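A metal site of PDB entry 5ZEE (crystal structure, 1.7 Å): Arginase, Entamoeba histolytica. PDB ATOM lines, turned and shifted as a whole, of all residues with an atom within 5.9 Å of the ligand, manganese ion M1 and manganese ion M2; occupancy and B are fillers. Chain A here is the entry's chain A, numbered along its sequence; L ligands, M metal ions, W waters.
The side-chain hydroxyl of Ser 153 lies within hydrogen-bond range of an oxygen (O1) of the ligand.
The side-chain hydroxyl (OG1) of Thr 255 lies within hydrogen-bond range of a nitrogen (N4) of the ligand (2.6 Å).
An oxygen (O3) of the ligand sits at hydrogen-bond distance from the side-chain amide nitrogen of Asn 146 (3.0 Å).
The side-chain carboxylate of Asp 194 lies within salt-bridge range of a nitrogen (N1) of the ligand, 3.0 Å away.
The side-chain carboxylate (OE2) of Glu 286 is in salt-bridge range of a nitrogen (N4) of the ligand (3.6 Å).
NE1 of Trp 138 sits close to OD2 of Asp 144.
OE2 of Glu 197 sits at hydrogen-bond distance from N of Asp 144 (3.0 Å).
The backbone NH (N) of Asp 241 lies within hydrogen-bond range of the backbone carbonyl oxygen (O) of Phe 139 (2.8 Å).
OD2 of Asp 243 sits close to OG1 of Thr 255.
The side-chain carboxylate (OD1) of Asp 243 lies close to the backbone NH (N) of Ala 141 (3.2 Å).
The backbone NH (N) of Ser 153 sits at hydrogen-bond distance from the side-chain hydroxyl (OG) of Ser 151 (3.1 Å).
The backbone NH (N) of Asp 194 sits at hydrogen-bond distance from the side-chain carboxylate (OE1) of Glu 197, at 2.8 Å.
A ring nitrogen (ND1) of His 157 sits at hydrogen-bond distance from the side-chain carboxylate (OE2) of Glu 286, at 2.8 Å.
Pro 152 touches the ligand (CD to O3, 3.8 Å).
CE1 of His 157 touches C6 of the ligand, at 3.3 Å.
CA of Gly 158 touches C5 of the ligand, 3.6 Å away.
Hydrophobic or aromatic side chains that line the ligand: His 114, His 142, Pro 152 and His 157.
Along chain A the residues within 4 Å of the ligand span positions 114 to 286.
The nearest printed residue that does not touch the ligand is Ser 151 (4.1 Å).
Within 4 Å of manganese ion M1: His 114, Asp 140, Asp 144 and Asp 241.
The nearest printed residue that does not touch manganese ion M1 is Trp 138 (4.03 Å).
Of the 25 residues printed, 4 come within 4 Å of manganese ion M2.
Manganese ion M1 is bound by an oxygen (O2) of the ligand (1.9 Å), the side-chain carboxylate (OD2) of Asp 140 (1.9 Å), a ring nitrogen (ND1) of His 114 (2.0 Å), the side-chain carboxylate (OD2) of Asp 144 (2.1 Å) and the side-chain carboxylate (OD2) of Asp 241 (2.3 Å).
O2 of the ligand is bound to manganese ion M2 (1.9 Å).
OD2 of Asp 241 is bound to manganese ion M2 (2.3 Å).
Manganese ion M2 is bound by OD1 of Asp 140, 2.3 Å away.
Manganese ion M2 is bound by the side-chain carboxylate (OD2) of Asp 243 (2.4 Å).
Manganese ion M2 is bound by a ring nitrogen (ND1) of His 142 (2.5 Å).
Manganese ion M2 is bound by the side-chain carboxylate (OD1) of Asp 243.
Manganese ion M2 has six donor atoms within binding distance.
Slightly farther from manganese ion M2 lies a nitrogen (N4) of the ligand (2.8 Å).
Water W4 lies within hydrogen-bond range of OG of Ser 151 (2.5 Å), O3 of the ligand (2.7 Å), O of Asn 155 (2.7 Å) and OG of Ser 153 (3.5 Å).
Water W3 lies within hydrogen-bond range of the backbone carbonyl oxygen of Ser 192 (2.6 Å), the side-chain carboxylate of Glu 197 (2.8 Å) and a nitrogen (N1) of the ligand (2.8 Å).
Water W5 lies within hydrogen-bond range of OE2 of Glu 197, N1 of the ligand, ND2 of Asn 146, O of Gly 158 and N of Asp 144.
Water W2 lies within hydrogen-bond range of NE2 of His 157 (2.7 Å), ND2 of Asn 155 (2.9 Å) and O1 of the ligand (3.2 Å).
Water W6 lies within hydrogen-bond range of OG1 of Thr 255 and N4 of the ligand.
Water W1 lies within hydrogen-bond range of OE1 of Glu 286, N4 of the ligand and OG1 of Thr 255.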
ATOM      1  N   HIS A 114       6.374  19.369   2.353  1.00  0.00           N
ATOM      2  CA  HIS A 114       6.443  20.690   3.002  1.00  0.00           C
ATOM      3  C   HIS A 114       5.299  21.624   2.673  1.00  0.00           C
ATOM      4  O   HIS A 114       5.189  22.692   3.300  1.00  0.00           O
ATOM      5  CB  HIS A 114       7.795  21.390   2.782  1.00  0.00           C
ATOM      6  CG  HIS A 114       8.283  22.125   3.985  1.00  0.00           C
ATOM      7  ND1 HIS A 114       9.595  22.511   4.129  1.00  0.00           N
ATOM      8  CD2 HIS A 114       7.655  22.456   5.139  1.00  0.00           C
ATOM      9  CE1 HIS A 114       9.731  23.112   5.303  1.00  0.00           C
ATOM     10  NE2 HIS A 114       8.576  23.062   5.950  1.00  0.00           N
ATOM     11  N   TRP A 138      13.007  28.094   9.559  1.00  0.00           N
ATOM     12  CA  TRP A 138      12.720  27.205   8.418  1.00  0.00           C
ATOM     13  C   TRP A 138      14.031  26.576   8.042  1.00  0.00           C
ATOM     14  O   TRP A 138      14.873  27.206   7.419  1.00  0.00           O
ATOM     15  CB  TRP A 138      12.118  28.028   7.293  1.00  0.00           C
ATOM     16  CG  TRP A 138      11.504  27.304   6.197  1.00  0.00           C
ATOM     17  CD1 TRP A 138      12.096  26.869   5.050  1.00  0.00           C
ATOM     18  CD2 TRP A 138      10.125  26.978   6.070  1.00  0.00           C
ATOM     19  NE1 TRP A 138      11.160  26.265   4.220  1.00  0.00           N
ATOM     20  CE2 TRP A 138       9.940  26.334   4.823  1.00  0.00           C
ATOM     21  CE3 TRP A 138       9.021  27.143   6.896  1.00  0.00           C
ATOM     22  CZ2 TRP A 138       8.660  25.856   4.384  1.00  0.00           C
ATOM     23  CZ3 TRP A 138       7.774  26.670   6.463  1.00  0.00           C
ATOM     24  CH2 TRP A 138       7.613  26.039   5.229  1.00  0.00           C
ATOM     25  N   PHE A 139      14.233  25.337   8.462  1.00  0.00           N
ATOM     26  CA  PHE A 139      15.444  24.586   8.182  1.00  0.00           C
ATOM     27  C   PHE A 139      15.185  23.751   6.937  1.00  0.00           C
ATOM     28  O   PHE A 139      14.301  22.892   6.914  1.00  0.00           O
ATOM     29  CB  PHE A 139      15.718  23.665   9.383  1.00  0.00           C
ATOM     30  CG  PHE A 139      16.946  22.819   9.259  1.00  0.00           C
ATOM     31  CD1 PHE A 139      16.956  21.614   8.536  1.00  0.00           C
ATOM     32  CD2 PHE A 139      18.117  23.199   9.926  1.00  0.00           C
ATOM     33  CE1 PHE A 139      18.096  20.800   8.451  1.00  0.00           C
ATOM     34  CE2 PHE A 139      19.252  22.416   9.841  1.00  0.00           C
ATOM     35  CZ  PHE A 139      19.245  21.205   9.132  1.00  0.00           C
ATOM     36  N   ASP A 140      15.974  23.988   5.894  1.00  0.00           N
ATOM     37  CA  ASP A 140      15.602  23.491   4.568  1.00  0.00           C
ATOM     38  C   ASP A 140      16.707  23.761   3.583  1.00  0.00           C
ATOM     39  O   ASP A 140      17.486  24.713   3.753  1.00  0.00           O
ATOM     40  CB  ASP A 140      14.358  24.275   4.131  1.00  0.00           C
ATOM     41  CG  ASP A 140      13.479  23.509   3.146  1.00  0.00           C
ATOM     42  OD1 ASP A 140      13.986  22.894   2.197  1.00  0.00           O
ATOM     43  OD2 ASP A 140      12.257  23.612   3.349  1.00  0.00           O
ATOM     44  N   ALA A 141      16.856  22.905   2.581  1.00  0.00           N
ATOM     45  CA  ALA A 141      17.642  23.273   1.369  1.00  0.00           C
ATOM     46  C   ALA A 141      16.977  24.379   0.496  1.00  0.00           C
ATOM     47  O   ALA A 141      17.671  25.089  -0.259  1.00  0.00           O
ATOM     48  CB  ALA A 141      17.925  22.059   0.545  1.00  0.00           C
ATOM     49  N   HIS A 142      15.650  24.535   0.630  1.00  0.00           N
ATOM     50  CA  HIS A 142      14.861  25.408  -0.224  1.00  0.00           C
ATOM     51  C   HIS A 142      14.127  26.488   0.590  1.00  0.00           C
ATOM     52  O   HIS A 142      13.623  26.209   1.658  1.00  0.00           O
ATOM     53  CB  HIS A 142      13.790  24.577  -0.951  1.00  0.00           C
ATOM     54  CG  HIS A 142      14.345  23.397  -1.638  1.00  0.00           C
ATOM     55  ND1 HIS A 142      14.361  22.150  -1.053  1.00  0.00           N
ATOM     56  CD2 HIS A 142      14.935  23.263  -2.848  1.00  0.00           C
ATOM     57  CE1 HIS A 142      14.985  21.306  -1.876  1.00  0.00           C
ATOM     58  NE2 HIS A 142      15.321  21.958  -2.981  1.00  0.00           N
ATOM     59  N   ASP A 144      11.225  27.761  -0.293  1.00  0.00           N
ATOM     60  CA  ASP A 144       9.792  27.446  -0.401  1.00  0.00           C
ATOM     61  C   ASP A 144       8.956  28.724  -0.480  1.00  0.00           C
ATOM     62  O   ASP A 144       7.867  28.829   0.101  1.00  0.00           O
ATOM     63  CB  ASP A 144       9.355  26.558   0.777  1.00  0.00           C
ATOM     64  CG  ASP A 144       9.941  25.143   0.710  1.00  0.00           C
ATOM     65  OD1 ASP A 144      10.432  24.781  -0.369  1.00  0.00           O
ATOM     66  OD2 ASP A 144       9.969  24.397   1.749  1.00  0.00           O
ATOM     67  N   ASN A 146       8.192  30.206  -3.726  1.00  0.00           N
ATOM     68  CA  ASN A 146       7.777  30.371  -5.100  1.00  0.00           C
ATOM     69  C   ASN A 146       6.263  30.586  -5.120  1.00  0.00           C
ATOM     70  O   ASN A 146       5.577  30.333  -4.138  1.00  0.00           O
ATOM     71  CB  ASN A 146       8.096  29.101  -5.889  1.00  0.00           C
ATOM     72  CG  ASN A 146       9.574  28.976  -6.236  1.00  0.00           C
ATOM     73  OD1 ASN A 146      10.230  29.964  -6.526  1.00  0.00           O
ATOM     74  ND2 ASN A 146      10.068  27.783  -6.239  1.00  0.00           N
ATOM     75  N   SER A 151       6.861  29.333 -10.343  1.00  0.00           N
ATOM     76  CA  SER A 151       7.304  27.999  -9.903  1.00  0.00           C
ATOM     77  C   SER A 151       7.854  27.219 -11.070  1.00  0.00           C
ATOM     78  O   SER A 151       7.214  27.170 -12.094  1.00  0.00           O
ATOM     79  CB  SER A 151       6.172  27.176  -9.295  1.00  0.00           C
ATOM     80  OG  SER A 151       6.628  25.849  -9.094  1.00  0.00           O
ATOM     81  N   PRO A 152       9.016  26.569 -10.917  1.00  0.00           N
ATOM     82  CA  PRO A 152       9.475  25.730 -12.045  1.00  0.00           C
ATOM     83  C   PRO A 152       8.754  24.408 -12.187  1.00  0.00           C
ATOM     84  O   PRO A 152       8.908  23.754 -13.190  1.00  0.00           O
ATOM     85  CB  PRO A 152      10.962  25.479 -11.706  1.00  0.00           C
ATOM     86  CG  PRO A 152      10.993  25.507 -10.212  1.00  0.00           C
ATOM     87  CD  PRO A 152       9.972  26.556  -9.789  1.00  0.00           C
ATOM     88  N   SER A 153       7.990  23.976 -11.183  1.00  0.00           N
ATOM     89  CA  SER A 153       7.394  22.657 -11.163  1.00  0.00           C
ATOM     90  C   SER A 153       5.865  22.632 -11.011  1.00  0.00           C
ATOM     91  O   SER A 153       5.243  21.622 -11.321  1.00  0.00           O
ATOM     92  CB  SER A 153       7.987  21.943  -9.943  1.00  0.00           C
ATOM     93  OG  SER A 153       7.616  22.604  -8.710  1.00  0.00           O
ATOM     94  N   GLY A 154       5.240  23.690 -10.493  1.00  0.00           N
ATOM     95  CA  GLY A 154       3.832  23.626 -10.061  1.00  0.00           C
ATOM     96  C   GLY A 154       3.560  22.887  -8.755  1.00  0.00           C
ATOM     97  O   GLY A 154       2.415  22.757  -8.323  1.00  0.00           O
ATOM     98  N   ASN A 155       4.630  22.443  -8.080  1.00  0.00           N
ATOM     99  CA  ASN A 155       4.537  21.656  -6.846  1.00  0.00           C
ATOM    100  C   ASN A 155       4.388  22.626  -5.655  1.00  0.00           C
ATOM    101  O   ASN A 155       5.243  23.448  -5.403  1.00  0.00           O
ATOM    102  CB  ASN A 155       5.754  20.781  -6.665  1.00  0.00           C
ATOM    103  CG  ASN A 155       5.842  19.663  -7.665  1.00  0.00           C
ATOM    104  OD1 ASN A 155       4.845  19.250  -8.272  1.00  0.00           O
ATOM    105  ND2 ASN A 155       7.058  19.130  -7.822  1.00  0.00           N
ATOM    106  N   HIS A 157       4.617  22.251  -2.569  1.00  0.00           N
ATOM    107  CA  HIS A 157       5.580  22.170  -1.477  1.00  0.00           C
ATOM    108  C   HIS A 157       6.695  23.185  -1.595  1.00  0.00           C
ATOM    109  O   HIS A 157       7.411  23.430  -0.605  1.00  0.00           O
ATOM    110  CB  HIS A 157       6.111  20.722  -1.273  1.00  0.00           C
ATOM    111  CG  HIS A 157       7.131  20.264  -2.257  1.00  0.00           C
ATOM    112  ND1 HIS A 157       7.985  19.208  -1.991  1.00  0.00           N
ATOM    113  CD2 HIS A 157       7.446  20.710  -3.491  1.00  0.00           C
ATOM    114  CE1 HIS A 157       8.789  19.042  -3.032  1.00  0.00           C
ATOM    115  NE2 HIS A 157       8.493  19.934  -3.955  1.00  0.00           N
ATOM    116  N   GLY A 158       6.778  23.847  -2.733  1.00  0.00           N
ATOM    117  CA  GLY A 158       7.752  24.887  -2.918  1.00  0.00           C
ATOM    118  C   GLY A 158       7.163  26.270  -2.743  1.00  0.00           C
ATOM    119  O   GLY A 158       7.810  27.228  -2.984  1.00  0.00           O
ATOM    120  N   MET A 159       5.931  26.340  -2.257  1.00  0.00           N
ATOM    121  CA  MET A 159       5.229  27.604  -2.082  1.00  0.00           C
ATOM    122  C   MET A 159       4.703  28.013  -0.703  1.00  0.00           C
ATOM    123  O   MET A 159       4.250  29.100  -0.556  1.00  0.00           O
ATOM    124  CB  MET A 159       4.017  27.614  -3.012  1.00  0.00           C
ATOM    125  CG  MET A 159       4.275  27.282  -4.459  1.00  0.00           C
ATOM    126  SD  MET A 159       2.728  27.258  -5.390  1.00  0.00           S
ATOM    127  CE  MET A 159       3.272  26.363  -6.805  1.00  0.00           C
ATOM    128  N   SER A 192      19.383  25.833  -2.535  1.00  0.00           N
ATOM    129  CA  SER A 192      18.812  25.689  -3.846  1.00  0.00           C
ATOM    130  C   SER A 192      17.755  26.775  -3.929  1.00  0.00           C
ATOM    131  O   SER A 192      16.671  26.609  -3.482  1.00  0.00           O
ATOM    132  CB  SER A 192      18.226  24.299  -4.052  1.00  0.00           C
ATOM    133  OG  SER A 192      17.532  24.202  -5.252  1.00  0.00           O
ATOM    134  N   ASP A 194      15.595  29.696  -6.195  1.00  0.00           N
ATOM    135  CA  ASP A 194      15.121  30.110  -7.496  1.00  0.00           C
ATOM    136  C   ASP A 194      15.138  31.619  -7.660  1.00  0.00           C
ATOM    137  O   ASP A 194      15.305  32.324  -6.718  1.00  0.00           O
ATOM    138  CB  ASP A 194      13.717  29.588  -7.754  1.00  0.00           C
ATOM    139  CG  ASP A 194      13.657  28.095  -7.901  1.00  0.00           C
ATOM    140  OD1 ASP A 194      14.623  27.484  -8.355  1.00  0.00           O
ATOM    141  OD2 ASP A 194      12.638  27.519  -7.583  1.00  0.00           O
ATOM    142  N   GLU A 197      12.776  33.595  -5.383  1.00  0.00           N
ATOM    143  CA  GLU A 197      13.124  33.445  -3.996  1.00  0.00           C
ATOM    144  C   GLU A 197      14.318  34.328  -3.639  1.00  0.00           C
ATOM    145  O   GLU A 197      14.323  34.969  -2.615  1.00  0.00           O
ATOM    146  CB  GLU A 197      13.397  31.995  -3.661  1.00  0.00           C
ATOM    147  CG  GLU A 197      12.177  31.088  -3.943  1.00  0.00           C
ATOM    148  CD  GLU A 197      12.503  29.626  -3.718  1.00  0.00           C
ATOM    149  OE1 GLU A 197      13.523  29.118  -4.327  1.00  0.00           O
ATOM    150  OE2 GLU A 197      11.746  28.990  -2.942  1.00  0.00           O
ATOM    151  N   ASP A 241      12.641  20.641   7.409  1.00  0.00           N
ATOM    152  CA  ASP A 241      12.722  19.829   6.232  1.00  0.00           C
ATOM    153  C   ASP A 241      14.020  19.062   6.273  1.00  0.00           C
ATOM    154  O   ASP A 241      15.121  19.623   6.308  1.00  0.00           O
ATOM    155  CB  ASP A 241      12.661  20.757   5.003  1.00  0.00           C
ATOM    156  CG  ASP A 241      12.464  20.020   3.686  1.00  0.00           C
ATOM    157  OD1 ASP A 241      12.950  18.860   3.548  1.00  0.00           O
ATOM    158  OD2 ASP A 241      11.870  20.651   2.759  1.00  0.00           O
ATOM    159  N   ASP A 243      15.630  17.595   4.110  1.00  0.00           N
ATOM    160  CA  ASP A 243      16.586  17.824   3.003  1.00  0.00           C
ATOM    161  C   ASP A 243      17.538  19.021   3.236  1.00  0.00           C
ATOM    162  O   ASP A 243      18.449  19.252   2.464  1.00  0.00           O
ATOM    163  CB  ASP A 243      15.911  17.870   1.646  1.00  0.00           C
ATOM    164  CG  ASP A 243      15.112  19.126   1.360  1.00  0.00           C
ATOM    165  OD1 ASP A 243      15.297  20.218   1.977  1.00  0.00           O
ATOM    166  OD2 ASP A 243      14.237  18.983   0.446  1.00  0.00           O
ATOM    167  N   GLY A 244      17.308  19.748   4.308  1.00  0.00           N
ATOM    168  CA  GLY A 244      18.352  20.672   4.830  1.00  0.00           C
ATOM    169  C   GLY A 244      19.662  19.962   5.094  1.00  0.00           C
ATOM    170  O   GLY A 244      20.765  20.532   4.930  1.00  0.00           O
ATOM    171  N   THR A 255      13.719  15.718  -2.920  1.00  0.00           N
ATOM    172  CA  THR A 255      14.530  16.730  -3.567  1.00  0.00           C
ATOM    173  C   THR A 255      15.843  16.947  -2.790  1.00  0.00           C
ATOM    174  O   THR A 255      16.040  18.019  -2.201  1.00  0.00           O
ATOM    175  CB  THR A 255      13.764  18.061  -3.663  1.00  0.00           C
ATOM    176  OG1 THR A 255      13.318  18.464  -2.358  1.00  0.00           O
ATOM    177  CG2 THR A 255      12.505  17.916  -4.586  1.00  0.00           C
ATOM    178  N   VAL A 285       9.377  17.233   8.159  1.00  0.00           N
ATOM    179  CA  VAL A 285       8.804  16.976   6.847  1.00  0.00           C
ATOM    180  C   VAL A 285       9.778  16.393   5.840  1.00  0.00           C
ATOM    181  O   VAL A 285      10.989  16.486   5.974  1.00  0.00           O
ATOM    182  CB  VAL A 285       8.188  18.253   6.249  1.00  0.00           C
ATOM    183  CG1 VAL A 285       7.079  18.825   7.144  1.00  0.00           C
ATOM    184  CG2 VAL A 285       9.228  19.303   5.908  1.00  0.00           C
ATOM    185  N   GLU A 286       9.180  15.776   4.817  1.00  0.00           N
ATOM    186  CA  GLU A 286       9.820  15.320   3.602  1.00  0.00           C
ATOM    187  C   GLU A 286      10.549  13.984   3.702  1.00  0.00           C
ATOM    188  O   GLU A 286      11.294  13.642   2.806  1.00  0.00           O
ATOM    189  CB  GLU A 286      10.684  16.421   2.933  1.00  0.00           C
ATOM    190  CG  GLU A 286       9.928  17.661   2.465  1.00  0.00           C
ATOM    191  CD  GLU A 286       9.105  17.465   1.136  1.00  0.00           C
ATOM    192  OE1 GLU A 286       9.130  16.368   0.509  1.00  0.00           O
ATOM    193  OE2 GLU A 286       8.473  18.462   0.661  1.00  0.00           O
HETATM  194  N1  LIG L   1      12.205  25.133  -5.827  1.00  0.00           N
HETATM  195  C1  LIG L   1      11.669  23.776  -6.206  1.00  0.00           C
HETATM  196  C2  LIG L   1      10.229  23.865  -6.749  1.00  0.00           C
HETATM  197  O1  LIG L   1       9.909  22.912  -7.510  1.00  0.00           O
HETATM  198  C3  LIG L   1      11.716  22.825  -5.019  1.00  0.00           C
HETATM  199  C4  LIG L   1      11.091  23.503  -3.776  1.00  0.00           C
HETATM  200  C5  LIG L   1      10.532  22.611  -2.692  1.00  0.00           C
HETATM  201  N2  LIG L   1      11.257  21.650  -2.190  1.00  0.00           N
HETATM  202  C6  LIG L   1      10.703  20.852  -1.094  1.00  0.00           C
HETATM  203  N3  LIG L   1      10.511  21.775   0.060  1.00  0.00           N
HETATM  204  N4  LIG L   1      11.531  19.690  -0.863  1.00  0.00           N
HETATM  205  O2  LIG L   1      11.582  22.143   0.901  1.00  0.00           O
HETATM  206  O3  LIG L   1       9.509  24.877  -6.405  1.00  0.00           O
HETATM  207 MN    MN M   1      10.778  22.616   2.562  1.00  0.00          MN
HETATM  208 MN    MN M   2      13.189  21.121   0.880  1.00  0.00          MN
HETATM  209  O   HOH W   1      10.507  16.564  -1.714  1.00  0.00           O
HETATM  210  O   HOH W   2       9.474  19.942  -6.446  1.00  0.00           O
HETATM  211  O   HOH W   3      14.161  26.435  -4.252  1.00  0.00           O
HETATM  212  O   HOH W   4       6.892  25.261  -6.627  1.00  0.00           O
HETATM  213  O   HOH W   5      11.024  26.571  -3.545  1.00  0.00           O
HETATM  214  O   HOH W   6      12.902  16.678  -0.325  1.00  0.00           O
